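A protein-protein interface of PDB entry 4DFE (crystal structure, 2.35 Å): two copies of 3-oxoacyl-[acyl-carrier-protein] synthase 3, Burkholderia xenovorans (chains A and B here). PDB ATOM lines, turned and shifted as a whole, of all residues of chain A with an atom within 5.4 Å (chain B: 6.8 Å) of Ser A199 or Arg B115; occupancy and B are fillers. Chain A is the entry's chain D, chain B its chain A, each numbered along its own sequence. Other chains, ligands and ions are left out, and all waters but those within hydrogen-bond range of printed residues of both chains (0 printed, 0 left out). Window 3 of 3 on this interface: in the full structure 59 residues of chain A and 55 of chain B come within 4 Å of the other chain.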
ATOM      1  N   ASP A 197      -3.228   0.969 -26.041  1.00  0.00           N
ATOM      2  CA  ASP A 197      -3.858   1.769 -24.986  1.00  0.00           C
ATOM      3  C   ASP A 197      -5.333   2.020 -25.294  1.00  0.00           C
ATOM      4  O   ASP A 197      -5.687   2.948 -26.033  1.00  0.00           O
ATOM      5  CB  ASP A 197      -3.115   3.114 -24.797  1.00  0.00           C
ATOM      6  CG  ASP A 197      -3.591   3.884 -23.567  1.00  0.00           C
ATOM      7  OD1 ASP A 197      -4.697   3.572 -23.043  1.00  0.00           O
ATOM      8  OD2 ASP A 197      -2.873   4.843 -23.158  1.00  0.00           O
ATOM      9  N   GLY A 198      -6.184   1.207 -24.692  1.00  0.00           N
ATOM     10  CA  GLY A 198      -7.604   1.256 -24.933  1.00  0.00           C
ATOM     11  C   GLY A 198      -8.294   2.505 -24.434  1.00  0.00           C
ATOM     12  O   GLY A 198      -9.445   2.757 -24.799  1.00  0.00           O
ATOM     13  N   SER A 199      -7.627   3.291 -23.597  1.00  0.00           N
ATOM     14  CA  SER A 199      -8.229   4.574 -23.148  1.00  0.00           C
ATOM     15  C   SER A 199      -8.435   5.555 -24.323  1.00  0.00           C
ATOM     16  O   SER A 199      -9.180   6.495 -24.218  1.00  0.00           O
ATOM     17  CB  SER A 199      -7.382   5.218 -22.032  1.00  0.00           C
ATOM     18  OG  SER A 199      -6.130   5.685 -22.520  1.00  0.00           O
ATOM     19  N   HIS A 200      -7.789   5.298 -25.453  1.00  0.00           N
ATOM     20  CA  HIS A 200      -7.940   6.162 -26.620  1.00  0.00           C
ATOM     21  C   HIS A 200      -8.744   5.505 -27.746  1.00  0.00           C
ATOM     22  O   HIS A 200      -8.593   5.847 -28.922  1.00  0.00           O
ATOM     23  CB  HIS A 200      -6.549   6.546 -27.116  1.00  0.00           C
ATOM     24  CG  HIS A 200      -5.698   7.265 -26.084  1.00  0.00           C
ATOM     25  ND1 HIS A 200      -6.129   8.379 -25.414  1.00  0.00           N
ATOM     26  CD2 HIS A 200      -4.406   7.013 -25.632  1.00  0.00           C
ATOM     27  CE1 HIS A 200      -5.158   8.809 -24.595  1.00  0.00           C
ATOM     28  NE2 HIS A 200      -4.095   7.981 -24.732  1.00  0.00           N
ATOM     29  N   SER A 201      -9.614   4.557 -27.384  1.00  0.00           N
ATOM     30  CA  SER A 201     -10.486   3.875 -28.359  1.00  0.00           C
ATOM     31  C   SER A 201     -11.470   4.838 -29.041  1.00  0.00           C
ATOM     32  O   SER A 201     -11.826   4.638 -30.193  1.00  0.00           O
ATOM     33  CB  SER A 201     -11.259   2.728 -27.707  1.00  0.00           C
ATOM     34  OG  SER A 201     -12.044   3.185 -26.622  1.00  0.00           O
ATOM     35  N   ASN A 202     -11.905   5.875 -28.333  1.00  0.00           N
ATOM     36  CA  ASN A 202     -13.009   6.694 -28.819  1.00  0.00           C
ATOM     37  C   ASN A 202     -12.615   7.654 -29.963  1.00  0.00           C
ATOM     38  O   ASN A 202     -13.477   8.135 -30.704  1.00  0.00           O
ATOM     39  CB  ASN A 202     -13.608   7.473 -27.677  1.00  0.00           C
ATOM     40  CG  ASN A 202     -12.841   8.723 -27.397  1.00  0.00           C
ATOM     41  OD1 ASN A 202     -13.200   9.778 -27.941  1.00  0.00           O
ATOM     42  ND2 ASN A 202     -11.714   8.622 -26.628  1.00  0.00           N
ATOM     43  N   GLY A 323      -7.458   1.522 -31.440  1.00  0.00           N
ATOM     44  CA  GLY A 323      -7.217   0.755 -30.255  1.00  0.00           C
ATOM     45  C   GLY A 323      -7.242   1.630 -29.026  1.00  0.00           C
ATOM     46  O   GLY A 323      -8.161   1.508 -28.230  1.00  0.00           O
ATOM     47  N   PRO B  84      -3.722  -5.644 -11.277  1.00  0.00           N
ATOM     48  CA  PRO B  84      -4.098  -5.533 -12.681  1.00  0.00           C
ATOM     49  C   PRO B  84      -3.013  -4.927 -13.577  1.00  0.00           C
ATOM     50  O   PRO B  84      -2.895  -5.306 -14.749  1.00  0.00           O
ATOM     51  CB  PRO B  84      -5.344  -4.637 -12.645  1.00  0.00           C
ATOM     52  CG  PRO B  84      -5.915  -4.793 -11.283  1.00  0.00           C
ATOM     53  CD  PRO B  84      -4.755  -5.089 -10.372  1.00  0.00           C
ATOM     54  N   GLN B  85      -2.203  -4.023 -13.041  1.00  0.00           N
ATOM     55  CA  GLN B  85      -1.147  -3.364 -13.816  1.00  0.00           C
ATOM     56  C   GLN B  85       0.003  -4.293 -14.204  1.00  0.00           C
ATOM     57  O   GLN B  85       0.884  -3.889 -14.964  1.00  0.00           O
ATOM     58  CB  GLN B  85      -0.578  -2.144 -13.043  1.00  0.00           C
ATOM     59  CG  GLN B  85      -1.634  -1.096 -12.628  1.00  0.00           C
ATOM     60  CD  GLN B  85      -2.509  -0.609 -13.784  1.00  0.00           C
ATOM     61  OE1 GLN B  85      -2.003  -0.309 -14.852  1.00  0.00           O
ATOM     62  NE2 GLN B  85      -3.818  -0.521 -13.567  1.00  0.00           N
ATOM     63  N   CYS B 106      -8.760  -4.290 -26.575  1.00  0.00           N
ATOM     64  CA  CYS B 106      -8.450  -2.910 -26.267  1.00  0.00           C
ATOM     65  C   CYS B 106      -9.481  -2.313 -25.361  1.00  0.00           C
ATOM     66  O   CYS B 106      -9.144  -1.572 -24.441  1.00  0.00           O
ATOM     67  CB  CYS B 106      -8.352  -2.084 -27.532  1.00  0.00           C
ATOM     68  SG  CYS B 106      -6.776  -2.237 -28.380  1.00  0.00           S
ATOM     69  N   GLN B 109      -9.003  -3.814 -21.906  1.00  0.00           N
ATOM     70  CA  GLN B 109      -7.854  -3.157 -21.259  1.00  0.00           C
ATOM     71  C   GLN B 109      -8.271  -1.908 -20.526  1.00  0.00           C
ATOM     72  O   GLN B 109      -7.884  -1.685 -19.372  1.00  0.00           O
ATOM     73  CB  GLN B 109      -6.776  -2.776 -22.285  1.00  0.00           C
ATOM     74  CG  GLN B 109      -5.397  -2.565 -21.672  1.00  0.00           C
ATOM     75  CD  GLN B 109      -4.441  -1.812 -22.591  1.00  0.00           C
ATOM     76  OE1 GLN B 109      -4.728  -0.693 -23.004  1.00  0.00           O
ATOM     77  NE2 GLN B 109      -3.324  -2.401 -22.899  1.00  0.00           N
ATOM     78  N   ASN B 110      -9.052  -1.067 -21.196  1.00  0.00           N
ATOM     79  CA  ASN B 110      -9.460   0.190 -20.612  1.00  0.00           C
ATOM     80  C   ASN B 110     -10.482  -0.048 -19.492  1.00  0.00           C
ATOM     81  O   ASN B 110     -10.430   0.597 -18.452  1.00  0.00           O
ATOM     82  CB  ASN B 110     -10.029   1.107 -21.659  1.00  0.00           C
ATOM     83  CG  ASN B 110     -10.423   2.452 -21.065  1.00  0.00           C
ATOM     84  OD1 ASN B 110      -9.626   3.095 -20.390  1.00  0.00           O
ATOM     85  ND2 ASN B 110     -11.671   2.851 -21.263  1.00  0.00           N
ATOM     86  N   LEU B 112     -10.623  -2.515 -17.504  1.00  0.00           N
ATOM     87  CA  LEU B 112      -9.827  -2.912 -16.349  1.00  0.00           C
ATOM     88  C   LEU B 112      -8.933  -1.807 -15.813  1.00  0.00           C
ATOM     89  O   LEU B 112      -8.243  -2.008 -14.810  1.00  0.00           O
ATOM     90  CB  LEU B 112      -8.980  -4.131 -16.705  1.00  0.00           C
ATOM     91  CG  LEU B 112      -9.751  -5.428 -16.913  1.00  0.00           C
ATOM     92  CD1 LEU B 112      -8.850  -6.422 -17.636  1.00  0.00           C
ATOM     93  CD2 LEU B 112     -10.228  -6.022 -15.582  1.00  0.00           C
ATOM     94  N   GLY B 113      -8.876  -0.656 -16.477  1.00  0.00           N
ATOM     95  CA  GLY B 113      -8.033   0.449 -16.002  1.00  0.00           C
ATOM     96  C   GLY B 113      -6.543   0.163 -16.080  1.00  0.00           C
ATOM     97  O   GLY B 113      -5.758   0.645 -15.225  1.00  0.00           O
ATOM     98  N   ILE B 114      -6.127  -0.617 -17.089  1.00  0.00           N
ATOM     99  CA  ILE B 114      -4.722  -0.988 -17.225  1.00  0.00           C
ATOM    100  C   ILE B 114      -4.024   0.083 -18.040  1.00  0.00           C
ATOM    101  O   ILE B 114      -4.385   0.343 -19.173  1.00  0.00           O
ATOM    102  CB  ILE B 114      -4.519  -2.390 -17.854  1.00  0.00           C
ATOM    103  CG1 ILE B 114      -5.027  -3.486 -16.909  1.00  0.00           C
ATOM    104  CG2 ILE B 114      -3.068  -2.615 -18.210  1.00  0.00           C
ATOM    105  CD1 ILE B 114      -5.244  -4.827 -17.582  1.00  0.00           C
ATOM    106  N   ARG B 115      -2.968   0.646 -17.453  1.00  0.00           N
ATOM    107  CA  ARG B 115      -2.310   1.836 -17.970  1.00  0.00           C
ATOM    108  C   ARG B 115      -0.887   1.571 -18.459  1.00  0.00           C
ATOM    109  O   ARG B 115      -0.152   2.495 -18.733  1.00  0.00           O
ATOM    110  CB  ARG B 115      -2.240   2.870 -16.837  1.00  0.00           C
ATOM    111  CG  ARG B 115      -3.581   3.390 -16.379  1.00  0.00           C
ATOM    112  CD  ARG B 115      -4.397   3.871 -17.604  1.00  0.00           C
ATOM    113  NE  ARG B 115      -3.502   4.445 -18.655  1.00  0.00           N
ATOM    114  CZ  ARG B 115      -3.835   5.394 -19.535  1.00  0.00           C
ATOM    115  NH1 ARG B 115      -5.025   6.008 -19.479  1.00  0.00           N
ATOM    116  NH2 ARG B 115      -2.938   5.785 -20.448  1.00  0.00           N
ATOM    117  N   ASN B 116      -0.504   0.305 -18.574  1.00  0.00           N
ATOM    118  CA  ASN B 116       0.906  -0.059 -18.877  1.00  0.00           C
ATOM    119  C   ASN B 116       1.237  -0.172 -20.386  1.00  0.00           C
ATOM    120  O   ASN B 116       2.320  -0.570 -20.754  1.00  0.00           O
ATOM    121  CB  ASN B 116       1.286  -1.352 -18.145  1.00  0.00           C
ATOM    122  CG  ASN B 116       0.478  -2.544 -18.596  1.00  0.00           C
ATOM    123  OD1 ASN B 116      -0.059  -2.570 -19.698  1.00  0.00           O
ATOM    124  ND2 ASN B 116       0.392  -3.551 -17.742  1.00  0.00           N
ATOM    125  N   HIS B 117       0.276   0.127 -21.231  1.00  0.00           N
ATOM    126  CA  HIS B 117       0.462   0.088 -22.680  1.00  0.00           C
ATOM    127  C   HIS B 117       0.741  -1.292 -23.259  1.00  0.00           C
ATOM    128  O   HIS B 117       1.255  -1.408 -24.345  1.00  0.00           O
ATOM    129  CB  HIS B 117       1.566   1.043 -23.122  1.00  0.00           C
ATOM    130  CG  HIS B 117       1.274   2.500 -22.880  1.00  0.00           C
ATOM    131  ND1 HIS B 117       2.231   3.453 -22.987  1.00  0.00           N
ATOM    132  CD2 HIS B 117       0.101   3.165 -22.517  1.00  0.00           C
ATOM    133  CE1 HIS B 117       1.694   4.664 -22.739  1.00  0.00           C
ATOM    134  NE2 HIS B 117       0.392   4.496 -22.470  1.00  0.00           N
ATOM    135  N   GLY B 118       0.421  -2.346 -22.526  1.00  0.00           N
ATOM    136  CA  GLY B 118       0.731  -3.706 -22.979  1.00  0.00           C
ATOM    137  C   GLY B 118      -0.052  -4.048 -24.227  1.00  0.00           C
ATOM    138  O   GLY B 118      -1.078  -3.422 -24.526  1.00  0.00           O
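No position is printed for both chains.
Of the 9 pairs that touch across the chains among the printed residues, none has its exchanged pair printed and touching as well.
OE1 of Gln B109 sits at hydrogen-bond distance from N of Gly A198 (2.9 Å).
NH2 of Arg B115 lies within salt-bridge range of OD2 of Asp A197 (2.9 Å).
The guanidinium group (NH1) of Arg B115 sits at hydrogen-bond distance from the side-chain hydroxyl (OG) of Ser A199.
The side-chain carboxylate (OD2) of Asp A197 is in hydrogen-bond range of a ring nitrogen (NE2) of His B117.
Among the printed residues, pairs that only touch across the chains: Gly A198 with Cys B106, Asp A197 with Gln B109, Ser A199 with Asn B110, Gly A323 with Cys B106 and Gly A198 with Asn B110.
The backbone NH of Arg B115 sits at hydrogen-bond distance from the side-chain amide oxygen of Gln B85, at 2.9 Å.
N of Ile B114 lies within hydrogen-bond range of O of Gln B109 (3.1 Å).
The side-chain amide nitrogen of Gln B109 is in hydrogen-bond range of the backbone carbonyl oxygen of Gly B118 (3.0 Å).
The side-chain hydroxyl (OG) of Ser A199 is in hydrogen-bond range of the side-chain carboxylate (OD1) of Asp A197 (2.6 Å).
O of Gly A198 sits at hydrogen-bond distance from OG of Ser A201 (3.2 Å).
The backbone carbonyl oxygen (O) of Gly A323 lies close to the backbone NH (N) of Ser A201.
Of the printed residues of chain B, Asp A197 touches Gln B109, Arg B115 and His B117.
Of the printed residues of chain A, Gln B109 touches Asp A197 and Gly A198.
Of the printed residues of chain A, Asn B110 touches Gly A198 and Ser A199.
Arg B115 touches just these residues of chain A: Asp A197 (2.9 Å) and Ser A199 (3.3 Å).
Asn B116 touches none of the printed residues of chain A.
Of the printed residues of chain A, His B117 touches Asp A197.
The nearest residue of chain B that does not touch Ser A199 is Gln B109 (5.0 Å).
The nearest residue of chain A that does not touch Arg B115 is His A200 (5.0 Å).
Of the 12 printed residues of chain B, 5 touch a printed residue of chain A.
Hydrophobic or aromatic side chains of chain B that line the printed part of chain A: His B117.
Of the 7 printed residues of chain A, 4 touch a printed residue of chain B.
Printed residues of chain A that touch a printed residue of chain B: Asp A197, Gly A198, Ser A199 and Gly A323.
Among the printed residues, 9 pairs touch across the chains.
Among the printed residues, Asp or Glu carboxylates within 4 Å of a Lys or Arg side-chain nitrogen of the other chain: Asp A197 with Arg B115.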
